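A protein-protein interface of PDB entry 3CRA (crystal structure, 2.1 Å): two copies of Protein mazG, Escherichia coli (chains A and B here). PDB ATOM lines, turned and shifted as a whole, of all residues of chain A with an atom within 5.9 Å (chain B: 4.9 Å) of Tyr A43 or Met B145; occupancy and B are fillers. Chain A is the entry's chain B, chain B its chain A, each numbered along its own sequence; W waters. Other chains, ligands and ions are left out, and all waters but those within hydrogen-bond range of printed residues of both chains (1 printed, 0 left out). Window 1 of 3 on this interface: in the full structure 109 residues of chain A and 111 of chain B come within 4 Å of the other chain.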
ATOM      1  N   PRO A  36      34.946  -2.091   7.578  1.00  0.00           N
ATOM      2  CA  PRO A  36      33.559  -2.129   8.072  1.00  0.00           C
ATOM      3  C   PRO A  36      32.494  -1.917   7.030  1.00  0.00           C
ATOM      4  O   PRO A  36      31.317  -2.282   7.251  1.00  0.00           O
ATOM      5  CB  PRO A  36      33.487  -0.934   9.036  1.00  0.00           C
ATOM      6  CG  PRO A  36      34.675  -0.134   8.798  1.00  0.00           C
ATOM      7  CD  PRO A  36      35.736  -1.123   8.355  1.00  0.00           C
ATOM      8  N   THR A  38      32.926  -2.927   3.789  1.00  0.00           N
ATOM      9  CA  THR A  38      32.881  -4.218   3.105  1.00  0.00           C
ATOM     10  C   THR A  38      31.882  -5.199   3.789  1.00  0.00           C
ATOM     11  O   THR A  38      31.098  -5.856   3.098  1.00  0.00           O
ATOM     12  CB  THR A  38      34.282  -4.859   2.963  1.00  0.00           C
ATOM     13  OG1 THR A  38      35.167  -3.952   2.312  1.00  0.00           O
ATOM     14  CG2 THR A  38      34.243  -6.099   2.126  1.00  0.00           C
ATOM     15  N   LEU A  39      31.896  -5.255   5.122  1.00  0.00           N
ATOM     16  CA  LEU A  39      30.962  -6.106   5.917  1.00  0.00           C
ATOM     17  C   LEU A  39      29.501  -5.671   5.816  1.00  0.00           C
ATOM     18  O   LEU A  39      28.598  -6.498   5.564  1.00  0.00           O
ATOM     19  CB  LEU A  39      31.381  -6.119   7.399  1.00  0.00           C
ATOM     20  CG  LEU A  39      30.653  -7.199   8.222  1.00  0.00           C
ATOM     21  CD1 LEU A  39      30.528  -8.535   7.422  1.00  0.00           C
ATOM     22  CD2 LEU A  39      31.337  -7.431   9.494  1.00  0.00           C
ATOM     23  N   GLU A  40      29.270  -4.375   6.003  1.00  0.00           N
ATOM     24  CA  GLU A  40      27.914  -3.812   5.851  1.00  0.00           C
ATOM     25  C   GLU A  40      27.368  -4.093   4.445  1.00  0.00           C
ATOM     26  O   GLU A  40      26.211  -4.513   4.304  1.00  0.00           O
ATOM     27  CB  GLU A  40      27.929  -2.310   6.115  1.00  0.00           C
ATOM     28  CG  GLU A  40      26.841  -1.434   5.377  1.00  0.00           C
ATOM     29  CD  GLU A  40      27.082   0.100   5.590  1.00  0.00           C
ATOM     30  OE1 GLU A  40      27.618   0.765   4.666  1.00  0.00           O
ATOM     31  OE2 GLU A  40      26.746   0.646   6.694  1.00  0.00           O
ATOM     32  N   GLU A  41      28.171  -3.867   3.408  1.00  0.00           N
ATOM     33  CA  GLU A  41      27.686  -3.995   2.011  1.00  0.00           C
ATOM     34  C   GLU A  41      27.433  -5.472   1.653  1.00  0.00           C
ATOM     35  O   GLU A  41      26.535  -5.812   0.865  1.00  0.00           O
ATOM     36  CB  GLU A  41      28.694  -3.407   1.029  1.00  0.00           C
ATOM     37  CG  GLU A  41      28.214  -3.438  -0.471  1.00  0.00           C
ATOM     38  CD  GLU A  41      26.910  -2.735  -0.649  1.00  0.00           C
ATOM     39  OE1 GLU A  41      26.729  -1.643  -0.031  1.00  0.00           O
ATOM     40  OE2 GLU A  41      26.040  -3.306  -1.351  1.00  0.00           O
ATOM     41  N   THR A  42      28.255  -6.344   2.195  1.00  0.00           N
ATOM     42  CA  THR A  42      28.043  -7.760   1.971  1.00  0.00           C
ATOM     43  C   THR A  42      26.678  -8.244   2.444  1.00  0.00           C
ATOM     44  O   THR A  42      26.020  -8.984   1.736  1.00  0.00           O
ATOM     45  CB  THR A  42      29.174  -8.578   2.488  1.00  0.00           C
ATOM     46  OG1 THR A  42      30.335  -8.242   1.697  1.00  0.00           O
ATOM     47  CG2 THR A  42      28.884 -10.072   2.341  1.00  0.00           C
ATOM     48  N   TYR A  43      26.220  -7.766   3.577  1.00  0.00           N
ATOM     49  CA  TYR A  43      24.877  -8.108   4.032  1.00  0.00           C
ATOM     50  C   TYR A  43      23.803  -7.516   3.111  1.00  0.00           C
ATOM     51  O   TYR A  43      22.752  -8.108   2.953  1.00  0.00           O
ATOM     52  CB  TYR A  43      24.669  -7.658   5.502  1.00  0.00           C
ATOM     53  CG  TYR A  43      25.461  -8.581   6.441  1.00  0.00           C
ATOM     54  CD1 TYR A  43      25.035  -9.884   6.697  1.00  0.00           C
ATOM     55  CD2 TYR A  43      26.652  -8.155   7.007  1.00  0.00           C
ATOM     56  CE1 TYR A  43      25.764 -10.734   7.523  1.00  0.00           C
ATOM     57  CE2 TYR A  43      27.378  -8.991   7.850  1.00  0.00           C
ATOM     58  CZ  TYR A  43      26.925 -10.264   8.087  1.00  0.00           C
ATOM     59  OH  TYR A  43      27.692 -11.084   8.893  1.00  0.00           O
ATOM     60  N   GLU A  44      24.058  -6.332   2.577  1.00  0.00           N
ATOM     61  CA  GLU A  44      23.148  -5.689   1.611  1.00  0.00           C
ATOM     62  C   GLU A  44      23.042  -6.596   0.370  1.00  0.00           C
ATOM     63  O   GLU A  44      21.955  -6.918  -0.079  1.00  0.00           O
ATOM     64  CB  GLU A  44      23.666  -4.321   1.183  1.00  0.00           C
ATOM     65  CG  GLU A  44      23.865  -3.266   2.222  1.00  0.00           C
ATOM     66  CD  GLU A  44      22.579  -2.806   2.831  1.00  0.00           C
ATOM     67  OE1 GLU A  44      21.506  -3.351   2.463  1.00  0.00           O
ATOM     68  OE2 GLU A  44      22.635  -1.900   3.697  1.00  0.00           O
ATOM     69  N   VAL A  45      24.181  -7.040  -0.145  1.00  0.00           N
ATOM     70  CA  VAL A  45      24.181  -7.932  -1.298  1.00  0.00           C
ATOM     71  C   VAL A  45      23.375  -9.181  -0.992  1.00  0.00           C
ATOM     72  O   VAL A  45      22.528  -9.575  -1.823  1.00  0.00           O
ATOM     73  CB  VAL A  45      25.620  -8.293  -1.787  1.00  0.00           C
ATOM     74  CG1 VAL A  45      25.598  -9.461  -2.727  1.00  0.00           C
ATOM     75  CG2 VAL A  45      26.312  -7.051  -2.407  1.00  0.00           C
ATOM     76  N   LEU A  46      23.607  -9.803   0.170  1.00  0.00           N
ATOM     77  CA  LEU A  46      22.878 -11.066   0.471  1.00  0.00           C
ATOM     78  C   LEU A  46      21.421 -10.799   0.657  1.00  0.00           C
ATOM     79  O   LEU A  46      20.607 -11.633   0.272  1.00  0.00           O
ATOM     80  CB  LEU A  46      23.365 -11.785   1.747  1.00  0.00           C
ATOM     81  CG  LEU A  46      24.844 -12.060   1.853  1.00  0.00           C
ATOM     82  CD1 LEU A  46      25.200 -12.649   3.227  1.00  0.00           C
ATOM     83  CD2 LEU A  46      25.390 -12.803   0.670  1.00  0.00           C
ATOM     84  N   ASP A  47      21.074  -9.649   1.235  1.00  0.00           N
ATOM     85  CA  ASP A  47      19.647  -9.357   1.378  1.00  0.00           C
ATOM     86  C   ASP A  47      18.914  -9.198  -0.012  1.00  0.00           C
ATOM     87  O   ASP A  47      17.755  -9.651  -0.204  1.00  0.00           O
ATOM     88  CB  ASP A  47      19.465  -8.068   2.136  1.00  0.00           C
ATOM     89  CG  ASP A  47      18.044  -7.939   2.697  1.00  0.00           C
ATOM     90  OD1 ASP A  47      17.565  -8.859   3.422  1.00  0.00           O
ATOM     91  OD2 ASP A  47      17.436  -6.915   2.417  1.00  0.00           O
ATOM     92  N   ALA A  48      19.593  -8.514  -0.939  1.00  0.00           N
ATOM     93  CA  ALA A  48      19.070  -8.279  -2.250  1.00  0.00           C
ATOM     94  C   ALA A  48      18.863  -9.594  -2.953  1.00  0.00           C
ATOM     95  O   ALA A  48      17.864  -9.737  -3.650  1.00  0.00           O
ATOM     96  CB  ALA A  48      20.005  -7.371  -3.048  1.00  0.00           C
ATOM     97  N   SER A 140      33.219 -15.981  10.346  1.00  0.00           N
ATOM     98  CA  SER A 140      32.042 -15.302   9.917  1.00  0.00           C
ATOM     99  C   SER A 140      30.811 -15.467  10.774  1.00  0.00           C
ATOM    100  O   SER A 140      29.801 -14.904  10.426  1.00  0.00           O
ATOM    101  CB  SER A 140      31.732 -15.637   8.428  1.00  0.00           C
ATOM    102  OG  SER A 140      31.028 -16.838   8.271  1.00  0.00           O
ATOM    103  N   PRO A 142      28.221 -14.402  13.653  1.00  0.00           N
ATOM    104  CA  PRO A 142      28.013 -13.148  14.368  1.00  0.00           C
ATOM    105  C   PRO A 142      29.000 -13.056  15.602  1.00  0.00           C
ATOM    106  O   PRO A 142      29.324 -14.047  16.183  1.00  0.00           O
ATOM    107  CB  PRO A 142      26.541 -13.208  14.743  1.00  0.00           C
ATOM    108  CG  PRO A 142      25.908 -14.066  13.525  1.00  0.00           C
ATOM    109  CD  PRO A 142      26.950 -15.078  13.295  1.00  0.00           C
ATOM    110  N   LEU B  39      29.726 -14.203   1.922  1.00  0.00           N
ATOM    111  CA  LEU B  39      29.839 -13.912   3.345  1.00  0.00           C
ATOM    112  C   LEU B  39      31.203 -14.426   3.887  1.00  0.00           C
ATOM    113  O   LEU B  39      31.960 -13.674   4.513  1.00  0.00           O
ATOM    114  CB  LEU B  39      28.685 -14.573   4.154  1.00  0.00           C
ATOM    115  CG  LEU B  39      28.713 -14.118   5.655  1.00  0.00           C
ATOM    116  CD1 LEU B  39      28.508 -12.621   5.771  1.00  0.00           C
ATOM    117  CD2 LEU B  39      27.681 -14.850   6.529  1.00  0.00           C
ATOM    118  N   TYR B  43      34.762 -11.985   5.155  1.00  0.00           N
ATOM    119  CA  TYR B  43      35.501 -12.049   6.441  1.00  0.00           C
ATOM    120  C   TYR B  43      36.958 -12.428   6.207  1.00  0.00           C
ATOM    121  O   TYR B  43      37.818 -12.018   6.970  1.00  0.00           O
ATOM    122  CB  TYR B  43      34.869 -13.021   7.387  1.00  0.00           C
ATOM    123  CG  TYR B  43      33.679 -12.451   8.095  1.00  0.00           C
ATOM    124  CD1 TYR B  43      32.426 -12.600   7.564  1.00  0.00           C
ATOM    125  CD2 TYR B  43      33.816 -11.768   9.312  1.00  0.00           C
ATOM    126  CE1 TYR B  43      31.329 -12.081   8.188  1.00  0.00           C
ATOM    127  CE2 TYR B  43      32.730 -11.245   9.939  1.00  0.00           C
ATOM    128  CZ  TYR B  43      31.491 -11.417   9.390  1.00  0.00           C
ATOM    129  OH  TYR B  43      30.401 -10.909  10.018  1.00  0.00           O
ATOM    130  N   PRO B 138      18.463  -5.399   6.441  1.00  0.00           N
ATOM    131  CA  PRO B 138      18.641  -6.804   6.145  1.00  0.00           C
ATOM    132  C   PRO B 138      18.247  -7.670   7.347  1.00  0.00           C
ATOM    133  O   PRO B 138      18.697  -7.444   8.488  1.00  0.00           O
ATOM    134  CB  PRO B 138      20.123  -6.878   5.811  1.00  0.00           C
ATOM    135  CG  PRO B 138      20.400  -5.548   5.146  1.00  0.00           C
ATOM    136  CD  PRO B 138      19.587  -4.579   5.942  1.00  0.00           C
ATOM    137  N   SER B 140      19.338 -10.634   7.575  1.00  0.00           N
ATOM    138  CA  SER B 140      20.568 -11.407   7.819  1.00  0.00           C
ATOM    139  C   SER B 140      21.599 -10.820   8.868  1.00  0.00           C
ATOM    140  O   SER B 140      22.574 -11.486   9.231  1.00  0.00           O
ATOM    141  CB  SER B 140      21.321 -11.573   6.499  1.00  0.00           C
ATOM    142  OG  SER B 140      21.583 -10.284   5.859  1.00  0.00           O
ATOM    143  N   LEU B 141      21.413  -9.586   9.313  1.00  0.00           N
ATOM    144  CA  LEU B 141      22.475  -8.876  10.063  1.00  0.00           C
ATOM    145  C   LEU B 141      22.811  -9.496  11.425  1.00  0.00           C
ATOM    146  O   LEU B 141      21.913  -9.803  12.184  1.00  0.00           O
ATOM    147  CB  LEU B 141      22.019  -7.448  10.277  1.00  0.00           C
ATOM    148  CG  LEU B 141      22.245  -6.462   9.136  1.00  0.00           C
ATOM    149  CD1 LEU B 141      21.861  -5.066   9.640  1.00  0.00           C
ATOM    150  CD2 LEU B 141      23.683  -6.447   8.587  1.00  0.00           C
ATOM    151  N   PRO B 142      24.096  -9.693  11.752  1.00  0.00           N
ATOM    152  CA  PRO B 142      24.455 -10.090  13.121  1.00  0.00           C
ATOM    153  C   PRO B 142      23.760  -9.154  14.106  1.00  0.00           C
ATOM    154  O   PRO B 142      23.503  -8.009  13.756  1.00  0.00           O
ATOM    155  CB  PRO B 142      25.938  -9.838  13.148  1.00  0.00           C
ATOM    156  CG  PRO B 142      26.386 -10.128  11.747  1.00  0.00           C
ATOM    157  CD  PRO B 142      25.295  -9.570  10.894  1.00  0.00           C
ATOM    158  N   ALA B 143      23.451  -9.633  15.310  1.00  0.00           N
ATOM    159  CA  ALA B 143      22.666  -8.871  16.282  1.00  0.00           C
ATOM    160  C   ALA B 143      23.186  -7.504  16.647  1.00  0.00           C
ATOM    161  O   ALA B 143      22.398  -6.545  16.776  1.00  0.00           O
ATOM    162  CB  ALA B 143      22.428  -9.709  17.568  1.00  0.00           C
ATOM    163  N   LEU B 144      24.497  -7.400  16.809  1.00  0.00           N
ATOM    164  CA  LEU B 144      25.093  -6.086  17.167  1.00  0.00           C
ATOM    165  C   LEU B 144      24.970  -5.054  16.035  1.00  0.00           C
ATOM    166  O   LEU B 144      24.690  -3.881  16.303  1.00  0.00           O
ATOM    167  CB  LEU B 144      26.571  -6.242  17.588  1.00  0.00           C
ATOM    168  CG  LEU B 144      26.869  -7.004  18.893  1.00  0.00           C
ATOM    169  CD1 LEU B 144      28.393  -7.364  19.011  1.00  0.00           C
ATOM    170  CD2 LEU B 144      26.466  -6.237  20.082  1.00  0.00           C
ATOM    171  N   MET B 145      25.231  -5.504  14.783  1.00  0.00           N
ATOM    172  CA  MET B 145      25.043  -4.713  13.565  1.00  0.00           C
ATOM    173  C   MET B 145      23.618  -4.277  13.433  1.00  0.00           C
ATOM    174  O   MET B 145      23.341  -3.110  13.225  1.00  0.00           O
ATOM    175  CB  MET B 145      25.433  -5.496  12.335  1.00  0.00           C
ATOM    176  CG  MET B 145      26.881  -5.795  12.294  1.00  0.00           C
ATOM    177  SD  MET B 145      27.440  -6.493  10.755  1.00  0.00           S
ATOM    178  CE  MET B 145      27.260  -5.035   9.693  1.00  0.00           C
ATOM    179  N   ARG B 146      22.678  -5.201  13.644  1.00  0.00           N
ATOM    180  CA  ARG B 146      21.263  -4.832  13.542  1.00  0.00           C
ATOM    181  C   ARG B 146      20.884  -3.840  14.621  1.00  0.00           C
ATOM    182  O   ARG B 146      20.140  -2.879  14.346  1.00  0.00           O
ATOM    183  CB  ARG B 146      20.394  -6.084  13.729  1.00  0.00           C
ATOM    184  CG  ARG B 146      18.966  -5.777  13.470  1.00  0.00           C
ATOM    185  CD  ARG B 146      17.963  -6.994  13.643  1.00  0.00           C
ATOM    186  NE  ARG B 146      16.685  -6.499  13.144  1.00  0.00           N
ATOM    187  CZ  ARG B 146      16.388  -6.489  11.848  1.00  0.00           C
ATOM    188  NH1 ARG B 146      17.240  -7.072  11.008  1.00  0.00           N
ATOM    189  NH2 ARG B 146      15.281  -5.913  11.413  1.00  0.00           N
ATOM    190  N   ALA B 147      21.329  -4.023  15.875  1.00  0.00           N
ATOM    191  CA  ALA B 147      20.884  -3.053  16.942  1.00  0.00           C
ATOM    192  C   ALA B 147      21.377  -1.649  16.648  1.00  0.00           C
ATOM    193  O   ALA B 147      20.683  -0.696  16.886  1.00  0.00           O
ATOM    194  CB  ALA B 147      21.338  -3.480  18.304  1.00  0.00           C
ATOM    195  N   GLN B 148      22.608  -1.535  16.159  1.00  0.00           N
ATOM    196  CA  GLN B 148      23.275  -0.262  15.937  1.00  0.00           C
ATOM    197  C   GLN B 148      22.611   0.417  14.768  1.00  0.00           C
ATOM    198  O   GLN B 148      22.354   1.652  14.791  1.00  0.00           O
ATOM    199  CB  GLN B 148      24.753  -0.517  15.634  1.00  0.00           C
ATOM    200  CG  GLN B 148      25.530   0.797  15.499  1.00  0.00           C
ATOM    201  CD  GLN B 148      26.950   0.791  16.067  1.00  0.00           C
ATOM    202  OE1 GLN B 148      27.608   1.820  16.053  1.00  0.00           O
ATOM    203  NE2 GLN B 148      27.435  -0.360  16.492  1.00  0.00           N
ATOM    204  N   LYS B 149      22.273  -0.390  13.753  1.00  0.00           N
ATOM    205  CA  LYS B 149      21.515   0.136  12.595  1.00  0.00           C
ATOM    206  C   LYS B 149      20.107   0.635  13.009  1.00  0.00           C
ATOM    207  O   LYS B 149      19.709   1.753  12.686  1.00  0.00           O
ATOM    208  CB  LYS B 149      21.416  -0.919  11.483  1.00  0.00           C
ATOM    209  CG  LYS B 149      20.737  -0.409  10.158  1.00  0.00           C
ATOM    210  CD  LYS B 149      20.940  -1.443   9.064  1.00  0.00           C
ATOM    211  CE  LYS B 149      22.347  -1.339   8.452  1.00  0.00           C
ATOM    212  NZ  LYS B 149      22.372  -0.020   7.690  1.00  0.00           N
ATOM    213  N   GLU B 215      29.836  -4.347  16.522  1.00  0.00           N
ATOM    214  CA  GLU B 215      30.140  -5.680  16.012  1.00  0.00           C
ATOM    215  C   GLU B 215      31.632  -5.793  15.715  1.00  0.00           C
ATOM    216  O   GLU B 215      32.296  -6.775  16.084  1.00  0.00           O
ATOM    217  CB  GLU B 215      29.294  -5.974  14.746  1.00  0.00           C
ATOM    218  CG  GLU B 215      29.632  -7.262  14.040  1.00  0.00           C
ATOM    219  CD  GLU B 215      28.842  -8.429  14.529  1.00  0.00           C
ATOM    220  OE1 GLU B 215      29.129  -9.569  14.161  1.00  0.00           O
ATOM    221  OE2 GLU B 215      27.914  -8.194  15.259  1.00  0.00           O
HETATM  222  O   HOH W   1      19.312 -10.355   4.840  1.00  0.00           O
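The side-chain hydroxyl (OH) of Tyr A43 sits at hydrogen-bond distance from the side-chain hydroxyl (OH) of Tyr B43 (2.9 Å).
The backbone carbonyl oxygen (O) of Pro B138 is in hydrogen-bond range of the guanidinium group (NH1) of Arg B146.
Tyr B43 touches Leu A39. CD1 of Leu B39 touches OH of Tyr A43 (3.6 Å). Tyr A43 touches Ser B140 (CD1 to OG, 3.6 Å). Leu B141 touches Tyr A43 (CD2 to CB, 3.5 Å). CG of Pro B142 touches OH of Tyr A43, 3.3 Å away. CE2 of Tyr A43 touches SD of Met B145, 3.8 Å away. Pro B138 touches Glu A44 (CG to OE1, 3.6 Å). Ser A140 touches Tyr B43. Pro B142 touches Pro A142 (CB to CB, 3.8 Å). OE1 of Glu B215 touches CA of Pro A142 (3.8 Å).
Tyr A43 touches just these residues of chain B: Leu B39, Tyr B43, Ser B140, Leu B141, Pro B142 and Met B145. Printed residues of chain A within 4 Å of Met B145: Tyr A43 (3.8 Å). Of the printed residues of chain B, Asp A47 touches Pro B138 (3.6 Å). Of the printed residues of chain B, Leu A39 touches Tyr B43. Of the printed residues of chain A, Tyr B43 touches Leu A39 (3.5 Å), Tyr A43 (2.9 Å) and Ser A140 (3.2 Å). Printed residues of chain B within 4 Å of Glu A44: Pro B138 (3.6 Å). Of the printed residues of chain A, Glu B215 touches Pro A142 (3.8 Å). Ala A48 touches none of the printed residues of chain B. Arg B146 touches none of the printed residues of chain A. The nearest residue of chain B that does not touch Tyr A43 is Pro B138 (4.1 Å). The nearest residue of chain A that does not touch Met B145 is Glu A40 (4.1 Å). The nearest printed residue of chain A that does not touch Pro B142 is Ser A140 (6.0 Å).
Hydrophobic or aromatic side chains of chain B that line the printed part of chain A: Leu B39, Tyr B43, Pro B138, Leu B141, Pro B142 and Met B145. Among the printed residues, 12 pairs touch across the chains. Among the printed residues, no Asp or Glu carboxylate lies within 4 Å of a Lys or Arg side-chain nitrogen of the other chain.
Leu A39 touches Tyr B43, and with the chains exchanged Tyr A43 touches Leu B39. Tyr A43 touches Ser B140, and with the chains exchanged Ser A140 touches Tyr B43. Tyr A43 touches Pro B142, but with the chains exchanged Pro A142 does not touch Tyr B43 (5.4 Å). Pro A142 touches its own counterpart, Pro B142. Positions printed for both chains: 39, 43, 140 and 142.
Water W1 bridges OG of Ser B140 (2.5 Å) and OD1 of Asp A47 (2.7 Å).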
